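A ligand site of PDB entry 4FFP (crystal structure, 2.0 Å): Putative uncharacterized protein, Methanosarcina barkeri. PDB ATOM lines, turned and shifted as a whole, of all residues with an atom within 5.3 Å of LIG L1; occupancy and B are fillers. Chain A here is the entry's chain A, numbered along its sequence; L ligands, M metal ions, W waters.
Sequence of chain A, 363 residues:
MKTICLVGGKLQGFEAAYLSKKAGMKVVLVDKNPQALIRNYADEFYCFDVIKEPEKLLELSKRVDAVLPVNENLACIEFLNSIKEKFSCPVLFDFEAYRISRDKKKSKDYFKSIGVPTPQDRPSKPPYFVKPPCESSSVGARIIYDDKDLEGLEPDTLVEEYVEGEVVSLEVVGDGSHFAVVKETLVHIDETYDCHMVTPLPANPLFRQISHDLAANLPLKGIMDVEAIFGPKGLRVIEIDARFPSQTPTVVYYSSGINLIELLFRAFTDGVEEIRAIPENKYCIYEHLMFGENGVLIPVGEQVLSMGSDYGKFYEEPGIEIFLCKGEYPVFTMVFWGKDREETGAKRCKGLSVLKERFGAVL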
ATOM      1  N   LYS A  10     -27.247 -23.611  -4.493  1.00  0.00           N
ATOM      2  CA  LYS A  10     -27.682 -22.327  -5.017  1.00  0.00           C
ATOM      3  C   LYS A  10     -28.079 -22.414  -6.478  1.00  0.00           C
ATOM      4  O   LYS A  10     -28.908 -23.241  -6.807  1.00  0.00           O
ATOM      5  CB  LYS A  10     -26.646 -21.268  -4.785  1.00  0.00           C
ATOM      6  CG  LYS A  10     -26.717 -20.750  -3.372  1.00  0.00           C
ATOM      7  CD  LYS A  10     -25.799 -19.577  -3.171  1.00  0.00           C
ATOM      8  CE  LYS A  10     -26.488 -18.233  -3.305  1.00  0.00           C
ATOM      9  NZ  LYS A  10     -25.516 -17.246  -2.762  1.00  0.00           N
ATOM     10  N   LEU A  11     -27.554 -21.557  -7.341  1.00  0.00           N
ATOM     11  CA  LEU A  11     -28.106 -21.486  -8.707  1.00  0.00           C
ATOM     12  C   LEU A  11     -27.727 -22.690  -9.578  1.00  0.00           C
ATOM     13  O   LEU A  11     -28.555 -23.239 -10.338  1.00  0.00           O
ATOM     14  CB  LEU A  11     -27.747 -20.159  -9.402  1.00  0.00           C
ATOM     15  CG  LEU A  11     -28.232 -18.879  -8.701  1.00  0.00           C
ATOM     16  CD1 LEU A  11     -27.763 -17.630  -9.429  1.00  0.00           C
ATOM     17  CD2 LEU A  11     -29.748 -18.874  -8.492  1.00  0.00           C
ATOM     18  N   GLN A  12     -26.450 -23.074  -9.504  1.00  0.00           N
ATOM     19  CA  GLN A  12     -25.987 -24.267 -10.218  1.00  0.00           C
ATOM     20  C   GLN A  12     -26.755 -25.458  -9.683  1.00  0.00           C
ATOM     21  O   GLN A  12     -27.164 -26.311 -10.442  1.00  0.00           O
ATOM     22  CB  GLN A  12     -24.488 -24.537 -10.008  1.00  0.00           C
ATOM     23  CG  GLN A  12     -23.525 -23.600 -10.713  1.00  0.00           C
ATOM     24  CD  GLN A  12     -22.119 -23.961 -10.320  1.00  0.00           C
ATOM     25  OE1 GLN A  12     -21.560 -23.423  -9.348  1.00  0.00           O
ATOM     26  NE2 GLN A  12     -21.590 -25.001 -10.956  1.00  0.00           N
ATOM     27  N   GLY A  13     -26.828 -25.536  -8.366  1.00  0.00           N
ATOM     28  CA  GLY A  13     -27.510 -26.612  -7.682  1.00  0.00           C
ATOM     29  C   GLY A  13     -28.947 -26.700  -8.166  1.00  0.00           C
ATOM     30  O   GLY A  13     -29.466 -27.812  -8.386  1.00  0.00           O
ATOM     31  N   VAL A  70     -21.559 -28.530  -7.496  1.00  0.00           N
ATOM     32  CA  VAL A  70     -22.223 -27.430  -8.161  1.00  0.00           C
ATOM     33  C   VAL A  70     -22.030 -26.186  -7.288  1.00  0.00           C
ATOM     34  O   VAL A  70     -22.977 -25.670  -6.721  1.00  0.00           O
ATOM     35  CB  VAL A  70     -23.720 -27.723  -8.426  1.00  0.00           C
ATOM     36  CG1 VAL A  70     -23.936 -28.365  -9.793  1.00  0.00           C
ATOM     37  CG2 VAL A  70     -24.310 -28.637  -7.360  1.00  0.00           C
ATOM     38  N   ASN A  71     -20.775 -25.781  -7.148  1.00  0.00           N
ATOM     39  CA  ASN A  71     -20.393 -24.563  -6.452  1.00  0.00           C
ATOM     40  C   ASN A  71     -19.060 -24.150  -7.046  1.00  0.00           C
ATOM     41  O   ASN A  71     -18.419 -24.922  -7.739  1.00  0.00           O
ATOM     42  CB  ASN A  71     -20.293 -24.785  -4.944  1.00  0.00           C
ATOM     43  CG  ASN A  71     -19.088 -25.618  -4.530  1.00  0.00           C
ATOM     44  OD1 ASN A  71     -17.982 -25.098  -4.420  1.00  0.00           O
ATOM     45  ND2 ASN A  71     -19.303 -26.899  -4.220  1.00  0.00           N
ATOM     46  N   GLU A  72     -18.655 -22.914  -6.768  1.00  0.00           N
ATOM     47  CA  GLU A  72     -17.440 -22.360  -7.287  1.00  0.00           C
ATOM     48  C   GLU A  72     -16.620 -21.910  -6.114  1.00  0.00           C
ATOM     49  O   GLU A  72     -15.879 -20.941  -6.192  1.00  0.00           O
ATOM     50  CB  GLU A  72     -17.762 -21.199  -8.215  1.00  0.00           C
ATOM     51  CG  GLU A  72     -18.449 -21.706  -9.471  1.00  0.00           C
ATOM     52  CD  GLU A  72     -18.959 -20.564 -10.335  1.00  0.00           C
ATOM     53  OE1 GLU A  72     -19.843 -19.820  -9.869  1.00  0.00           O
ATOM     54  OE2 GLU A  72     -18.481 -20.430 -11.474  1.00  0.00           O
ATOM     55  N   SER A 136     -17.946 -15.085 -11.316  1.00  0.00           N
ATOM     56  CA  SER A 136     -18.922 -15.536 -12.290  1.00  0.00           C
ATOM     57  C   SER A 136     -20.119 -14.599 -12.111  1.00  0.00           C
ATOM     58  O   SER A 136     -20.033 -13.627 -11.330  1.00  0.00           O
ATOM     59  CB  SER A 136     -19.308 -17.013 -12.080  1.00  0.00           C
ATOM     60  OG  SER A 136     -19.722 -17.246 -10.747  1.00  0.00           O
ATOM     61  N   SER A 137     -21.206 -14.901 -12.831  1.00  0.00           N
ATOM     62  CA  SER A 137     -22.457 -14.084 -12.828  1.00  0.00           C
ATOM     63  C   SER A 137     -22.300 -12.597 -13.173  1.00  0.00           C
ATOM     64  O   SER A 137     -23.195 -11.782 -12.830  1.00  0.00           O
ATOM     65  CB  SER A 137     -23.236 -14.161 -11.490  1.00  0.00           C
ATOM     66  OG  SER A 137     -23.508 -15.487 -11.112  1.00  0.00           O
ATOM     67  N   SER A 169     -24.030 -18.586 -26.014  1.00  0.00           N
ATOM     68  CA  SER A 169     -23.496 -19.644 -25.160  1.00  0.00           C
ATOM     69  C   SER A 169     -23.665 -21.016 -25.808  1.00  0.00           C
ATOM     70  O   SER A 169     -24.685 -21.281 -26.436  1.00  0.00           O
ATOM     71  CB  SER A 169     -24.246 -19.671 -23.822  1.00  0.00           C
ATOM     72  OG  SER A 169     -23.745 -20.716 -23.019  1.00  0.00           O
ATOM     73  N   GLU A 171     -22.926 -25.274 -24.644  1.00  0.00           N
ATOM     74  CA  GLU A 171     -22.344 -26.241 -23.710  1.00  0.00           C
ATOM     75  C   GLU A 171     -21.703 -27.365 -24.482  1.00  0.00           C
ATOM     76  O   GLU A 171     -22.154 -27.711 -25.584  1.00  0.00           O
ATOM     77  CB  GLU A 171     -23.398 -26.862 -22.807  1.00  0.00           C
ATOM     78  CG  GLU A 171     -23.749 -26.048 -21.557  1.00  0.00           C
ATOM     79  CD  GLU A 171     -24.581 -24.820 -21.872  1.00  0.00           C
ATOM     80  OE1 GLU A 171     -25.558 -24.950 -22.640  1.00  0.00           O
ATOM     81  OE2 GLU A 171     -24.233 -23.721 -21.359  1.00  0.00           O
ATOM     82  N   VAL A 187     -27.832 -15.099 -24.702  1.00  0.00           N
ATOM     83  CA  VAL A 187     -27.802 -14.651 -23.316  1.00  0.00           C
ATOM     84  C   VAL A 187     -28.273 -13.235 -23.356  1.00  0.00           C
ATOM     85  O   VAL A 187     -27.581 -12.381 -23.889  1.00  0.00           O
ATOM     86  CB  VAL A 187     -26.383 -14.708 -22.739  1.00  0.00           C
ATOM     87  CG1 VAL A 187     -26.309 -14.083 -21.327  1.00  0.00           C
ATOM     88  CG2 VAL A 187     -25.895 -16.148 -22.689  1.00  0.00           C
ATOM     89  N   CYS A 195     -27.395 -11.850 -16.578  1.00  0.00           N
ATOM     90  CA  CYS A 195     -28.321 -12.498 -17.511  1.00  0.00           C
ATOM     91  C   CYS A 195     -29.739 -12.625 -16.897  1.00  0.00           C
ATOM     92  O   CYS A 195     -29.901 -13.314 -15.888  1.00  0.00           O
ATOM     93  CB  CYS A 195     -27.758 -13.863 -17.954  1.00  0.00           C
ATOM     94  SG  CYS A 195     -28.940 -14.821 -18.926  1.00  0.00           S
ATOM     95  N   ASP A 225     -19.140 -24.732 -20.409  1.00  0.00           N
ATOM     96  CA  ASP A 225     -19.828 -23.913 -21.359  1.00  0.00           C
ATOM     97  C   ASP A 225     -18.860 -22.884 -21.931  1.00  0.00           C
ATOM     98  O   ASP A 225     -17.782 -22.616 -21.371  1.00  0.00           O
ATOM     99  CB  ASP A 225     -21.109 -23.327 -20.776  1.00  0.00           C
ATOM    100  CG  ASP A 225     -20.834 -22.258 -19.783  1.00  0.00           C
ATOM    101  OD1 ASP A 225     -21.690 -21.382 -19.575  1.00  0.00           O
ATOM    102  OD2 ASP A 225     -19.730 -22.277 -19.230  1.00  0.00           O
ATOM    103  N   GLU A 227     -18.651 -19.089 -23.838  1.00  0.00           N
ATOM    104  CA  GLU A 227     -19.434 -17.893 -24.116  1.00  0.00           C
ATOM    105  C   GLU A 227     -18.665 -17.023 -25.068  1.00  0.00           C
ATOM    106  O   GLU A 227     -17.455 -16.809 -24.857  1.00  0.00           O
ATOM    107  CB  GLU A 227     -19.691 -17.076 -22.849  1.00  0.00           C
ATOM    108  CG  GLU A 227     -20.342 -17.844 -21.697  1.00  0.00           C
ATOM    109  CD  GLU A 227     -20.967 -16.972 -20.606  1.00  0.00           C
ATOM    110  OE1 GLU A 227     -20.232 -16.488 -19.689  1.00  0.00           O
ATOM    111  OE2 GLU A 227     -22.202 -16.800 -20.663  1.00  0.00           O
ATOM    112  N   ARG A 243     -17.904 -26.203 -15.462  1.00  0.00           N
ATOM    113  CA  ARG A 243     -18.769 -26.572 -14.352  1.00  0.00           C
ATOM    114  C   ARG A 243     -20.209 -26.563 -14.855  1.00  0.00           C
ATOM    115  O   ARG A 243     -20.467 -26.060 -15.967  1.00  0.00           O
ATOM    116  CB  ARG A 243     -18.550 -25.723 -13.078  1.00  0.00           C
ATOM    117  CG  ARG A 243     -18.307 -24.219 -13.210  1.00  0.00           C
ATOM    118  CD  ARG A 243     -19.604 -23.549 -13.660  1.00  0.00           C
ATOM    119  NE  ARG A 243     -19.620 -22.111 -13.430  1.00  0.00           N
ATOM    120  CZ  ARG A 243     -20.192 -21.235 -14.246  1.00  0.00           C
ATOM    121  NH1 ARG A 243     -20.740 -21.616 -15.406  1.00  0.00           N
ATOM    122  NH2 ARG A 243     -20.138 -19.957 -13.920  1.00  0.00           N
ATOM    123  N   PRO A 245     -23.585 -25.347 -15.677  1.00  0.00           N
ATOM    124  CA  PRO A 245     -24.108 -23.983 -15.664  1.00  0.00           C
ATOM    125  C   PRO A 245     -25.549 -23.843 -15.173  1.00  0.00           C
ATOM    126  O   PRO A 245     -26.287 -24.825 -15.088  1.00  0.00           O
ATOM    127  CB  PRO A 245     -24.103 -23.600 -17.131  1.00  0.00           C
ATOM    128  CG  PRO A 245     -24.197 -24.874 -17.897  1.00  0.00           C
ATOM    129  CD  PRO A 245     -23.571 -25.939 -17.029  1.00  0.00           C
ATOM    130  N   SER A 246     -25.964 -22.591 -14.966  1.00  0.00           N
ATOM    131  CA  SER A 246     -27.348 -22.271 -14.676  1.00  0.00           C
ATOM    132  C   SER A 246     -28.000 -21.612 -15.905  1.00  0.00           C
ATOM    133  O   SER A 246     -27.315 -21.127 -16.831  1.00  0.00           O
ATOM    134  CB  SER A 246     -27.426 -21.337 -13.456  1.00  0.00           C
ATOM    135  OG  SER A 246     -26.721 -20.144 -13.773  1.00  0.00           O
ATOM    136  N   GLN A 247     -29.321 -21.674 -15.918  1.00  0.00           N
ATOM    137  CA  GLN A 247     -30.175 -20.986 -16.898  1.00  0.00           C
ATOM    138  C   GLN A 247     -30.132 -21.656 -18.270  1.00  0.00           C
ATOM    139  O   GLN A 247     -31.128 -22.219 -18.728  1.00  0.00           O
ATOM    140  CB  GLN A 247     -29.865 -19.465 -17.020  1.00  0.00           C
ATOM    141  CG  GLN A 247     -29.742 -18.705 -15.705  1.00  0.00           C
ATOM    142  CD  GLN A 247     -29.353 -17.264 -15.937  1.00  0.00           C
ATOM    143  OE1 GLN A 247     -28.289 -16.983 -16.496  1.00  0.00           O
ATOM    144  NE2 GLN A 247     -30.204 -16.338 -15.551  1.00  0.00           N
ATOM    145  N   THR A 248     -29.003 -21.637 -18.946  1.00  0.00           N
ATOM    146  CA  THR A 248     -28.997 -22.210 -20.289  1.00  0.00           C
ATOM    147  C   THR A 248     -29.436 -23.688 -20.369  1.00  0.00           C
ATOM    148  O   THR A 248     -30.050 -24.088 -21.349  1.00  0.00           O
ATOM    149  CB  THR A 248     -27.636 -22.005 -21.004  1.00  0.00           C
ATOM    150  OG1 THR A 248     -26.583 -22.544 -20.205  1.00  0.00           O
ATOM    151  CG2 THR A 248     -27.356 -20.519 -21.234  1.00  0.00           C
ATOM    152  N   GLU A 302     -29.404 -13.207 -12.299  1.00  0.00           N
ATOM    153  CA  GLU A 302     -28.983 -14.180 -11.310  1.00  0.00           C
ATOM    154  C   GLU A 302     -28.455 -13.629 -10.042  1.00  0.00           C
ATOM    155  O   GLU A 302     -28.625 -14.271  -9.018  1.00  0.00           O
ATOM    156  CB  GLU A 302     -27.846 -15.042 -11.835  1.00  0.00           C
ATOM    157  CG  GLU A 302     -28.216 -15.855 -13.024  1.00  0.00           C
ATOM    158  CD  GLU A 302     -27.368 -17.065 -13.169  1.00  0.00           C
ATOM    159  OE1 GLU A 302     -26.154 -16.922 -13.435  1.00  0.00           O
ATOM    160  OE2 GLU A 302     -27.922 -18.149 -12.943  1.00  0.00           O
ATOM    161  N   SER A 306     -29.866 -14.965  -6.415  1.00  0.00           N
ATOM    162  CA  SER A 306     -29.026 -15.668  -5.500  1.00  0.00           C
ATOM    163  C   SER A 306     -29.011 -15.039  -4.096  1.00  0.00           C
ATOM    164  O   SER A 306     -28.321 -15.527  -3.196  1.00  0.00           O
ATOM    165  CB  SER A 306     -27.616 -15.710  -6.054  1.00  0.00           C
ATOM    166  OG  SER A 306     -26.996 -14.511  -5.653  1.00  0.00           O
HETATM  167  O1  LIG L   1     -24.122 -20.368 -15.760  1.00  0.00           O
HETATM  168  C1  LIG L   1     -24.200 -19.195 -15.405  1.00  0.00           C
HETATM  169  C2  LIG L   1     -24.643 -18.126 -16.405  1.00  0.00           C
HETATM  170  C3  LIG L   1     -24.272 -18.267 -17.927  1.00  0.00           C
HETATM  171  C4  LIG L   1     -24.156 -19.733 -18.396  1.00  0.00           C
HETATM  172  C5  LIG L   1     -24.275 -19.915 -19.932  1.00  0.00           C
HETATM  173  N1  LIG L   1     -24.120 -21.354 -20.221  1.00  0.00           N
HETATM  174  N2  LIG L   1     -26.113 -18.086 -16.262  1.00  0.00           N
HETATM  175  N3  LIG L   1     -24.012 -18.742 -14.107  1.00  0.00           N
HETATM  176  C6  LIG L   1     -23.455 -19.529 -12.971  1.00  0.00           C
HETATM  177  C7  LIG L   1     -23.529 -18.774 -11.608  1.00  0.00           C
HETATM  178  C8  LIG L   1     -23.486 -19.706 -10.347  1.00  0.00           C
HETATM  179  C9  LIG L   1     -22.906 -19.011  -9.088  1.00  0.00           C
HETATM  180  C10 LIG L   1     -22.808 -19.916  -7.820  1.00  0.00           C
HETATM  181  N4  LIG L   1     -21.737 -20.899  -8.047  1.00  0.00           N
HETATM  182  C11 LIG L   1     -24.125 -20.620  -7.520  1.00  0.00           C
HETATM  183  O2  LIG L   1     -24.181 -21.868  -7.714  1.00  0.00           O
HETATM  184  O3  LIG L   1     -25.129 -19.948  -7.122  1.00  0.00           O
HETATM  185  P1  LG2 L   2     -21.855 -18.073  -3.646  1.00  0.00           P
HETATM  186  O1  LG2 L   2     -22.897 -17.339  -4.445  1.00  0.00           O
HETATM  187  O2  LG2 L   2     -20.480 -17.454  -3.815  1.00  0.00           O
HETATM  188  O3  LG2 L   2     -22.243 -18.354  -2.203  1.00  0.00           O
HETATM  189  P2  LG2 L   2     -20.730 -20.674  -4.254  1.00  0.00           P
HETATM  190  O4  LG2 L   2     -19.470 -20.407  -3.459  1.00  0.00           O
HETATM  191  O5  LG2 L   2     -20.653 -21.235  -5.658  1.00  0.00           O
HETATM  192  O6  LG2 L   2     -21.814 -19.499  -4.397  1.00  0.00           O
HETATM  193  O7  LG2 L   2     -21.524 -21.773  -3.372  1.00  0.00           O
HETATM  194  C1  LG2 L   2     -22.756 -22.314  -3.846  1.00  0.00           C
HETATM  195  C2  LG2 L   2     -23.355 -23.209  -2.772  1.00  0.00           C
HETATM  196  O8  LG2 L   2     -22.431 -24.266  -2.497  1.00  0.00           O
HETATM  197  C3  LG2 L   2     -23.590 -22.404  -1.506  1.00  0.00           C
HETATM  198  O9  LG2 L   2     -24.950 -22.615  -1.106  1.00  0.00           O
HETATM  199  C4  LG2 L   2     -22.577 -22.990  -0.546  1.00  0.00           C
HETATM  200  O10 LG2 L   2     -23.090 -22.870   0.785  1.00  0.00           O
HETATM  201  C5  LG2 L   2     -22.330 -24.414  -1.082  1.00  0.00           C
HETATM  202  N1  LG2 L   2     -20.982 -24.772  -0.697  1.00  0.00           N
HETATM  203  C6  LG2 L   2     -19.866 -24.082  -1.039  1.00  0.00           C
HETATM  204  N2  LG2 L   2     -18.800 -24.679  -0.428  1.00  0.00           N
HETATM  205  C7  LG2 L   2     -19.272 -25.722   0.298  1.00  0.00           C
HETATM  206  C8  LG2 L   2     -18.711 -26.788   1.138  1.00  0.00           C
HETATM  207  N3  LG2 L   2     -17.417 -26.881   1.458  1.00  0.00           N
HETATM  208  N4  LG2 L   2     -19.583 -27.682   1.648  1.00  0.00           N
HETATM  209  C9  LG2 L   2     -20.899 -27.678   1.448  1.00  0.00           C
HETATM  210  N5  LG2 L   2     -21.477 -26.757   0.702  1.00  0.00           N
HETATM  211  C10 LG2 L   2     -20.713 -25.806   0.096  1.00  0.00           C
HETATM  212 MG    MG M   1     -20.050 -15.282 -18.186  1.00  0.00          MG
HETATM  213  O   HOH W   1     -25.161 -23.992  -6.436  1.00  0.00           O
HETATM  214  O   HOH W   2     -24.707 -17.368  -6.574  1.00  0.00           O
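The side-chain hydroxyl of Ser 169 sits at hydrogen-bond distance from a nitrogen (N1) of LIG L1 (2.9 Å).
The side-chain carboxylate of Asp 225 is in salt-bridge range of a nitrogen (N1) of LIG L1.
OE1 of Glu 302 lies within salt-bridge range of N2 of LIG L1 (3.1 Å).
The side-chain amide oxygen (OE1) of Gln 247 is in hydrogen-bond range of a nitrogen (N2) of LIG L1, 2.5 Å away.
N3 of LIG L1 is in hydrogen-bond range of OG of Ser 246 (3.1 Å).
N of Glu 72 lies within hydrogen-bond range of O5 of LG2 L2 (2.8 Å).
N1 of LIG L1 lies within hydrogen-bond range of OG1 of Thr 248 (2.7 Å).
N4 of LIG L1 is in salt-bridge range of OE1 of Glu 72 (2.8 Å).
N of Ser 246 is in hydrogen-bond range of O1 of LIG L1 (3.0 Å).
NZ of Lys 10 lies within salt-bridge range of O1 of LG2 L2, 3.1 Å away.
The backbone NH (N) of Leu 11 is in hydrogen-bond range of an oxygen (O3) of LIG L1 (2.9 Å).
The side-chain amide oxygen (OE1) of Gln 12 is in hydrogen-bond range of a nitrogen (N4) of LIG L1 (2.8 Å).
The backbone carbonyl oxygen (O) of Ser 246 lies within hydrogen-bond range of a nitrogen (N2) of LIG L1 (3.3 Å).
OE2 of Glu 171 is in salt-bridge range of N1 of LIG L1 (2.6 Å).
The backbone NH (N) of Gln 12 sits at hydrogen-bond distance from an oxygen (O2) of LIG L1.
O5 of LG2 L2 lies within hydrogen-bond range of N4 of LIG L1 (2.6 Å).
OE2 of Glu 171 lies within hydrogen-bond range of OG1 of Thr 248, at 2.9 Å.
NE of Arg 243 is in salt-bridge range of OE2 of Glu 72, at 2.8 Å.
NE2 of Gln 247 sits at hydrogen-bond distance from O of Cys 195 (3.1 Å).
The backbone carbonyl oxygen of Ser 306 lies close to the side-chain amino group of Lys 10 (3.3 Å).
OG of Ser 169 is in hydrogen-bond range of OE2 of Glu 171, at 3.5 Å.
OE1 of Gln 12 sits at hydrogen-bond distance from N of Asn 71.
OG of Ser 136 lies within hydrogen-bond range of OE1 of Glu 72 (2.7 Å).
The side-chain hydroxyl of Ser 246 is in hydrogen-bond range of the side-chain carboxylate of Glu 302 (2.5 Å).
Lys 10 touches LIG L1.
OG of Ser 137 touches C7 of LIG L1, at 3.3 Å.
Glu 227 touches LIG L1.
Arg 243 touches LIG L1.
Pro 245 touches LIG L1.
Hydrophobic or aromatic side chains that line LIG L1: Leu 11 and Pro 245.
The nearest printed residue that does not touch LIG L1 is Ser 136 (4.001 Å).
Water W2 bridges O3 of LIG L1 and O1 of LG2 L2.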
